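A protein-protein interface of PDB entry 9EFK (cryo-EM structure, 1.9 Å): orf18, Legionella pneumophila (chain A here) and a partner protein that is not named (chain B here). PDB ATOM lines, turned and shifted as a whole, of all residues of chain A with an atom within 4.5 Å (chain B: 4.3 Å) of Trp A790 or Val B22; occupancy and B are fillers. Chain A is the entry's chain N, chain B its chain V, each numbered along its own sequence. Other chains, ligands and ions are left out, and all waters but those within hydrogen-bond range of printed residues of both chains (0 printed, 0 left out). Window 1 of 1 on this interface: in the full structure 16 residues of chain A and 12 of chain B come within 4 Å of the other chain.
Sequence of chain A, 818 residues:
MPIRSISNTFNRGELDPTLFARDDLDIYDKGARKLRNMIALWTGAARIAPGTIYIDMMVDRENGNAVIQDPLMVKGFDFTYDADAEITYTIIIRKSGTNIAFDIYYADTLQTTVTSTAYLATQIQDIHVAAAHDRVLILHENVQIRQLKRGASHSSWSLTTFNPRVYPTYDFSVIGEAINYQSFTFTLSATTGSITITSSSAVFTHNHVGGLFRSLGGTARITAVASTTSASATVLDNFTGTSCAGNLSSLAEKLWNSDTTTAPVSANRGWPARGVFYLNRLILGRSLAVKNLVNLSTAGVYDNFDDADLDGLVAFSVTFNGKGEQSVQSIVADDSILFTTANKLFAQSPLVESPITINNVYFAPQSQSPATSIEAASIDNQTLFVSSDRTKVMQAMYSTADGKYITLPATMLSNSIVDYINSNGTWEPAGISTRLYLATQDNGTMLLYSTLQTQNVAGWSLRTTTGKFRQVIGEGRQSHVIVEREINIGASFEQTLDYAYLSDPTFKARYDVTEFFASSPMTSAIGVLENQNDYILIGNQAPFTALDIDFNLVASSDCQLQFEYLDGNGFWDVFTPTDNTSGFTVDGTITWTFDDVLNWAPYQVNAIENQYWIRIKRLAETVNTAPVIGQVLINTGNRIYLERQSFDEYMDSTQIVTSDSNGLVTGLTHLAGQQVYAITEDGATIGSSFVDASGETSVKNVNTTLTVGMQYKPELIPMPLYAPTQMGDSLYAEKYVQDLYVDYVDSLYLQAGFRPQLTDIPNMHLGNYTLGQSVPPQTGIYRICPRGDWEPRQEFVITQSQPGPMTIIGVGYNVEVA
Hydrophobic or aromatic side chains of chain B that line the printed part of chain A: Met B156.
Of the 10 printed residues of chain A, 6 touch a printed residue of chain B.
Hydrophobic or aromatic side chains of chain A within 4 Å of the printed part of chain B: Tyr A736, Trp A790 and Ala A818.
Among the printed residues, 9 pairs touch across the chains.
Among the printed residues, no Asp or Glu carboxylate lies within 4 Å of a Lys or Arg side-chain nitrogen of the other chain.
Among the printed residues, pairs that only touch across the chains: Glu A734 with Thr B151 (3.4 Å), Ala A818 with Thr B151 (3.4 Å), Trp A790 with Thr B151 (3.6 Å), Trp A790 with Met B156 (3.6 Å), Ala A818 with Ser B153 (3.7 Å) and Asp A789 with Lys B24 (3.8 Å).
Trp A790 touches just these residues of chain B: Val B22, Thr B151 and Met B156.
Printed residues of chain B within 4 Å of Glu A816: Ser B153.
Val B22 touches just one residue of chain A: Trp A790 (3.0 Å).
Of the printed residues of chain A, Gly B23 touches Tyr A736.
Of the printed residues of chain A, Met B156 touches Trp A790 (3.6 Å).
The nearest printed residue of chain A that does not touch Ser B153 is Trp A790 (4.02 Å).
The backbone carbonyl oxygen (O) of Glu A734 lies within hydrogen-bond range of the backbone NH (N) of Ala A818, at 2.9 Å.
The backbone NH (N) of Lys A735 is in hydrogen-bond range of the backbone carbonyl oxygen (O) of Trp A790, at 3.4 Å.
O of Tyr A736 sits at hydrogen-bond distance from N of Glu A816, at 2.8 Å.
OD1 of Asp A789 is in hydrogen-bond range of N of Glu A791.
The backbone carbonyl oxygen of Ile B19 is in hydrogen-bond range of the backbone NH of Lys B24 (3.2 Å).
The side-chain hydroxyl of Ser B20 lies close to the backbone carbonyl oxygen of Lys B24, at 3.3 Å.
The backbone carbonyl oxygen (O) of Gly B23 lies within hydrogen-bond range of the side-chain hydroxyl (OH) of Tyr A736.
The backbone carbonyl oxygen (O) of Val B22 lies within hydrogen-bond range of the indole nitrogen (NE1) of Trp A790 (3.0 Å).
The side-chain carboxylate (OE2) of Glu A816 sits at hydrogen-bond distance from the side-chain hydroxyl (OG) of Ser B153, at 3.3 Å.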
ATOM      1  N   GLU A 734     -17.491   7.269   6.923  1.00  0.00           N
ATOM      2  CA  GLU A 734     -17.844   7.857   5.638  1.00  0.00           C
ATOM      3  C   GLU A 734     -16.708   7.649   4.647  1.00  0.00           C
ATOM      4  O   GLU A 734     -15.547   7.920   4.954  1.00  0.00           O
ATOM      5  CB  GLU A 734     -18.134   9.348   5.802  1.00  0.00           C
ATOM      6  CG  GLU A 734     -19.240   9.682   6.789  1.00  0.00           C
ATOM      7  CD  GLU A 734     -18.739   9.860   8.218  1.00  0.00           C
ATOM      8  OE1 GLU A 734     -17.538   9.637   8.474  1.00  0.00           O
ATOM      9  OE2 GLU A 734     -19.551  10.228   9.088  1.00  0.00           O
ATOM     10  N   LYS A 735     -17.044   7.159   3.458  1.00  0.00           N
ATOM     11  CA  LYS A 735     -16.063   6.873   2.422  1.00  0.00           C
ATOM     12  C   LYS A 735     -16.539   7.422   1.089  1.00  0.00           C
ATOM     13  O   LYS A 735     -17.734   7.436   0.802  1.00  0.00           O
ATOM     14  CB  LYS A 735     -15.822   5.378   2.261  1.00  0.00           C
ATOM     15  CG  LYS A 735     -15.416   4.658   3.507  1.00  0.00           C
ATOM     16  CD  LYS A 735     -15.181   3.205   3.198  1.00  0.00           C
ATOM     17  CE  LYS A 735     -15.204   2.379   4.450  1.00  0.00           C
ATOM     18  NZ  LYS A 735     -16.528   2.473   5.108  1.00  0.00           N
ATOM     19  N   TYR A 736     -15.590   7.848   0.266  1.00  0.00           N
ATOM     20  CA  TYR A 736     -15.881   8.296  -1.087  1.00  0.00           C
ATOM     21  C   TYR A 736     -14.889   7.658  -2.044  1.00  0.00           C
ATOM     22  O   TYR A 736     -13.685   7.655  -1.779  1.00  0.00           O
ATOM     23  CB  TYR A 736     -15.821   9.819  -1.196  1.00  0.00           C
ATOM     24  CG  TYR A 736     -16.095  10.331  -2.584  1.00  0.00           C
ATOM     25  CD1 TYR A 736     -17.390  10.438  -3.063  1.00  0.00           C
ATOM     26  CD2 TYR A 736     -15.058  10.702  -3.420  1.00  0.00           C
ATOM     27  CE1 TYR A 736     -17.641  10.902  -4.333  1.00  0.00           C
ATOM     28  CE2 TYR A 736     -15.299  11.167  -4.684  1.00  0.00           C
ATOM     29  CZ  TYR A 736     -16.589  11.263  -5.139  1.00  0.00           C
ATOM     30  OH  TYR A 736     -16.818  11.727  -6.407  1.00  0.00           O
ATOM     31  N   ASP A 789     -21.760   8.408  -3.566  1.00  0.00           N
ATOM     32  CA  ASP A 789     -22.022   9.180  -2.364  1.00  0.00           C
ATOM     33  C   ASP A 789     -20.966   8.892  -1.297  1.00  0.00           C
ATOM     34  O   ASP A 789     -19.904   8.331  -1.570  1.00  0.00           O
ATOM     35  CB  ASP A 789     -23.442   8.914  -1.861  1.00  0.00           C
ATOM     36  CG  ASP A 789     -23.684   7.463  -1.510  1.00  0.00           C
ATOM     37  OD1 ASP A 789     -22.744   6.649  -1.573  1.00  0.00           O
ATOM     38  OD2 ASP A 789     -24.835   7.132  -1.172  1.00  0.00           O
ATOM     39  N   TRP A 790     -21.251   9.304  -0.063  1.00  0.00           N
ATOM     40  CA  TRP A 790     -20.330   9.138   1.052  1.00  0.00           C
ATOM     41  C   TRP A 790     -20.794   8.078   2.047  1.00  0.00           C
ATOM     42  O   TRP A 790     -20.273   8.018   3.163  1.00  0.00           O
ATOM     43  CB  TRP A 790     -20.113  10.476   1.757  1.00  0.00           C
ATOM     44  CG  TRP A 790     -19.267  11.427   0.972  1.00  0.00           C
ATOM     45  CD1 TRP A 790     -19.658  12.188  -0.087  1.00  0.00           C
ATOM     46  CD2 TRP A 790     -17.884  11.715   1.184  1.00  0.00           C
ATOM     47  NE1 TRP A 790     -18.606  12.929  -0.549  1.00  0.00           N
ATOM     48  CE2 TRP A 790     -17.504  12.660   0.216  1.00  0.00           C
ATOM     49  CE3 TRP A 790     -16.930  11.267   2.099  1.00  0.00           C
ATOM     50  CZ2 TRP A 790     -16.213  13.163   0.136  1.00  0.00           C
ATOM     51  CZ3 TRP A 790     -15.653  11.767   2.018  1.00  0.00           C
ATOM     52  CH2 TRP A 790     -15.304  12.705   1.045  1.00  0.00           C
ATOM     53  N   GLU A 791     -21.747   7.239   1.668  1.00  0.00           N
ATOM     54  CA  GLU A 791     -22.284   6.242   2.584  1.00  0.00           C
ATOM     55  C   GLU A 791     -21.295   5.093   2.780  1.00  0.00           C
ATOM     56  O   GLU A 791     -20.618   4.691   1.833  1.00  0.00           O
ATOM     57  CB  GLU A 791     -23.606   5.695   2.064  1.00  0.00           C
ATOM     58  CG  GLU A 791     -24.734   6.702   2.088  1.00  0.00           C
ATOM     59  CD  GLU A 791     -25.117   7.112   3.494  1.00  0.00           C
ATOM     60  OE1 GLU A 791     -24.988   6.279   4.414  1.00  0.00           O
ATOM     61  OE2 GLU A 791     -25.545   8.268   3.682  1.00  0.00           O
ATOM     62  N   PRO A 792     -21.201   4.547   3.994  1.00  0.00           N
ATOM     63  CA  PRO A 792     -20.287   3.416   4.217  1.00  0.00           C
ATOM     64  C   PRO A 792     -20.622   2.181   3.400  1.00  0.00           C
ATOM     65  O   PRO A 792     -19.709   1.429   3.044  1.00  0.00           O
ATOM     66  CB  PRO A 792     -20.420   3.153   5.723  1.00  0.00           C
ATOM     67  CG  PRO A 792     -21.708   3.758   6.107  1.00  0.00           C
ATOM     68  CD  PRO A 792     -21.888   4.949   5.229  1.00  0.00           C
ATOM     69  N   GLN A 794     -22.141   1.744   0.065  1.00  0.00           N
ATOM     70  CA  GLN A 794     -22.596   2.131  -1.256  1.00  0.00           C
ATOM     71  C   GLN A 794     -22.262   1.016  -2.234  1.00  0.00           C
ATOM     72  O   GLN A 794     -21.275   0.298  -2.069  1.00  0.00           O
ATOM     73  CB  GLN A 794     -21.941   3.440  -1.690  1.00  0.00           C
ATOM     74  CG  GLN A 794     -20.488   3.535  -1.295  1.00  0.00           C
ATOM     75  CD  GLN A 794     -19.885   4.874  -1.628  1.00  0.00           C
ATOM     76  OE1 GLN A 794     -20.188   5.460  -2.663  1.00  0.00           O
ATOM     77  NE2 GLN A 794     -19.034   5.375  -0.747  1.00  0.00           N
ATOM     78  N   GLU A 816     -11.226   7.792  -0.402  1.00  0.00           N
ATOM     79  CA  GLU A 816     -10.999   8.805   0.619  1.00  0.00           C
ATOM     80  C   GLU A 816     -11.776   8.387   1.862  1.00  0.00           C
ATOM     81  O   GLU A 816     -13.010   8.408   1.866  1.00  0.00           O
ATOM     82  CB  GLU A 816     -11.430  10.179   0.112  1.00  0.00           C
ATOM     83  CG  GLU A 816     -11.686  11.221   1.190  1.00  0.00           C
ATOM     84  CD  GLU A 816     -10.432  11.646   1.926  1.00  0.00           C
ATOM     85  OE1 GLU A 816      -9.327  11.489   1.371  1.00  0.00           O
ATOM     86  OE2 GLU A 816     -10.552  12.139   3.065  1.00  0.00           O
ATOM     87  N   ALA A 818     -12.937   9.076   5.426  1.00  0.00           N
ATOM     88  CA  ALA A 818     -13.143  10.173   6.361  1.00  0.00           C
ATOM     89  C   ALA A 818     -13.691   9.661   7.685  1.00  0.00           C
ATOM     90  O   ALA A 818     -14.672  10.191   8.207  1.00  0.00           O
ATOM     91  CB  ALA A 818     -14.082  11.206   5.765  1.00  0.00           C
ATOM     92  OXT ALA A 818     -13.174   8.707   8.262  1.00  0.00           O
ATOM     93  N   ALA B  18     -24.154  21.921  -5.857  1.00  0.00           N
ATOM     94  CA  ALA B  18     -23.395  21.754  -4.621  1.00  0.00           C
ATOM     95  C   ALA B  18     -23.163  20.282  -4.306  1.00  0.00           C
ATOM     96  O   ALA B  18     -22.085  19.902  -3.840  1.00  0.00           O
ATOM     97  CB  ALA B  18     -24.116  22.441  -3.465  1.00  0.00           C
ATOM     98  N   ILE B  19     -24.166  19.440  -4.550  1.00  0.00           N
ATOM     99  CA  ILE B  19     -24.013  18.007  -4.328  1.00  0.00           C
ATOM    100  C   ILE B  19     -22.970  17.426  -5.275  1.00  0.00           C
ATOM    101  O   ILE B  19     -22.176  16.561  -4.893  1.00  0.00           O
ATOM    102  CB  ILE B  19     -25.372  17.302  -4.473  1.00  0.00           C
ATOM    103  CG1 ILE B  19     -26.308  17.735  -3.346  1.00  0.00           C
ATOM    104  CG2 ILE B  19     -25.198  15.800  -4.485  1.00  0.00           C
ATOM    105  CD1 ILE B  19     -27.715  17.243  -3.510  1.00  0.00           C
ATOM    106  N   SER B  20     -22.955  17.891  -6.523  1.00  0.00           N
ATOM    107  CA  SER B  20     -21.926  17.444  -7.452  1.00  0.00           C
ATOM    108  C   SER B  20     -20.545  17.926  -7.041  1.00  0.00           C
ATOM    109  O   SER B  20     -19.552  17.243  -7.301  1.00  0.00           O
ATOM    110  CB  SER B  20     -22.246  17.914  -8.866  1.00  0.00           C
ATOM    111  OG  SER B  20     -23.251  17.110  -9.442  1.00  0.00           O
ATOM    112  N   MET B  21     -20.454  19.089  -6.399  1.00  0.00           N
ATOM    113  CA  MET B  21     -19.149  19.593  -5.994  1.00  0.00           C
ATOM    114  C   MET B  21     -18.501  18.680  -4.961  1.00  0.00           C
ATOM    115  O   MET B  21     -17.280  18.495  -4.968  1.00  0.00           O
ATOM    116  CB  MET B  21     -19.276  21.018  -5.458  1.00  0.00           C
ATOM    117  CG  MET B  21     -17.971  21.597  -4.954  1.00  0.00           C
ATOM    118  SD  MET B  21     -17.898  23.389  -5.064  1.00  0.00           S
ATOM    119  CE  MET B  21     -17.897  23.596  -6.840  1.00  0.00           C
ATOM    120  N   VAL B  22     -19.297  18.087  -4.075  1.00  0.00           N
ATOM    121  CA  VAL B  22     -18.749  17.197  -3.059  1.00  0.00           C
ATOM    122  C   VAL B  22     -18.694  15.770  -3.587  1.00  0.00           C
ATOM    123  O   VAL B  22     -18.378  14.837  -2.843  1.00  0.00           O
ATOM    124  CB  VAL B  22     -19.542  17.281  -1.740  1.00  0.00           C
ATOM    125  CG1 VAL B  22     -19.474  18.684  -1.183  1.00  0.00           C
ATOM    126  CG2 VAL B  22     -20.976  16.856  -1.938  1.00  0.00           C
ATOM    127  N   GLY B  23     -19.003  15.587  -4.871  1.00  0.00           N
ATOM    128  CA  GLY B  23     -18.632  14.383  -5.587  1.00  0.00           C
ATOM    129  C   GLY B  23     -19.744  13.446  -6.008  1.00  0.00           C
ATOM    130  O   GLY B  23     -19.443  12.407  -6.599  1.00  0.00           O
ATOM    131  N   LYS B  24     -21.006  13.757  -5.750  1.00  0.00           N
ATOM    132  CA  LYS B  24     -22.091  12.835  -6.055  1.00  0.00           C
ATOM    133  C   LYS B  24     -22.846  13.268  -7.304  1.00  0.00           C
ATOM    134  O   LYS B  24     -23.165  14.447  -7.469  1.00  0.00           O
ATOM    135  CB  LYS B  24     -23.065  12.720  -4.885  1.00  0.00           C
ATOM    136  CG  LYS B  24     -24.195  11.758  -5.156  1.00  0.00           C
ATOM    137  CD  LYS B  24     -25.129  11.640  -3.981  1.00  0.00           C
ATOM    138  CE  LYS B  24     -26.436  11.015  -4.404  1.00  0.00           C
ATOM    139  NZ  LYS B  24     -26.201   9.759  -5.147  1.00  0.00           N
ATOM    140  N   LEU B  37     -27.225  13.518   1.370  1.00  0.00           N
ATOM    141  CA  LEU B  37     -26.774  14.774   0.781  1.00  0.00           C
ATOM    142  C   LEU B  37     -27.952  15.657   0.392  1.00  0.00           C
ATOM    143  O   LEU B  37     -27.920  16.872   0.607  1.00  0.00           O
ATOM    144  CB  LEU B  37     -25.886  14.500  -0.428  1.00  0.00           C
ATOM    145  CG  LEU B  37     -24.445  14.110  -0.116  1.00  0.00           C
ATOM    146  CD1 LEU B  37     -23.723  13.722  -1.381  1.00  0.00           C
ATOM    147  CD2 LEU B  37     -23.737  15.259   0.566  1.00  0.00           C
ATOM    148  N   ALA B 143     -21.871  23.759  -0.451  1.00  0.00           N
ATOM    149  CA  ALA B 143     -21.040  22.562  -0.459  1.00  0.00           C
ATOM    150  C   ALA B 143     -20.156  22.494   0.774  1.00  0.00           C
ATOM    151  O   ALA B 143     -19.886  21.405   1.285  1.00  0.00           O
ATOM    152  CB  ALA B 143     -20.186  22.520  -1.723  1.00  0.00           C
ATOM    153  N   THR B 151     -20.029  14.602   4.687  1.00  0.00           N
ATOM    154  CA  THR B 151     -18.803  13.889   4.337  1.00  0.00           C
ATOM    155  C   THR B 151     -17.927  13.627   5.553  1.00  0.00           C
ATOM    156  O   THR B 151     -17.212  12.620   5.589  1.00  0.00           O
ATOM    157  CB  THR B 151     -18.006  14.660   3.286  1.00  0.00           C
ATOM    158  OG1 THR B 151     -17.273  15.715   3.918  1.00  0.00           O
ATOM    159  CG2 THR B 151     -18.930  15.248   2.238  1.00  0.00           C
ATOM    160  N   SER B 153     -15.255  15.057   6.307  1.00  0.00           N
ATOM    161  CA  SER B 153     -13.899  14.999   5.780  1.00  0.00           C
ATOM    162  C   SER B 153     -13.220  16.344   5.977  1.00  0.00           C
ATOM    163  O   SER B 153     -13.656  17.351   5.413  1.00  0.00           O
ATOM    164  CB  SER B 153     -13.912  14.616   4.301  1.00  0.00           C
ATOM    165  OG  SER B 153     -12.605  14.624   3.762  1.00  0.00           O
ATOM    166  N   MET B 156     -11.845  17.537   2.561  1.00  0.00           N
ATOM    167  CA  MET B 156     -12.804  18.214   1.694  1.00  0.00           C
ATOM    168  C   MET B 156     -13.013  19.660   2.114  1.00  0.00           C
ATOM    169  O   MET B 156     -13.070  20.557   1.266  1.00  0.00           O
ATOM    170  CB  MET B 156     -14.132  17.462   1.695  1.00  0.00           C
ATOM    171  CG  MET B 156     -14.066  16.112   1.022  1.00  0.00           C
ATOM    172  SD  MET B 156     -13.765  16.253  -0.740  1.00  0.00           S
ATOM    173  CE  MET B 156     -15.318  16.950  -1.275  1.00  0.00           C
ATOM    174  N   ILE B 160     -12.415  23.083  -0.281  1.00  0.00           N
ATOM    175  CA  ILE B 160     -13.513  23.949  -0.691  1.00  0.00           C
ATOM    176  C   ILE B 160     -13.305  25.378  -0.205  1.00  0.00           C
ATOM    177  O   ILE B 160     -13.803  26.324  -0.822  1.00  0.00           O
ATOM    178  CB  ILE B 160     -14.845  23.370  -0.187  1.00  0.00           C
ATOM    179  CG1 ILE B 160     -15.068  21.976  -0.766  1.00  0.00           C
ATOM    180  CG2 ILE B 160     -16.011  24.259  -0.562  1.00  0.00           C
ATOM    181  CD1 ILE B 160     -16.280  21.282  -0.213  1.00  0.00           C
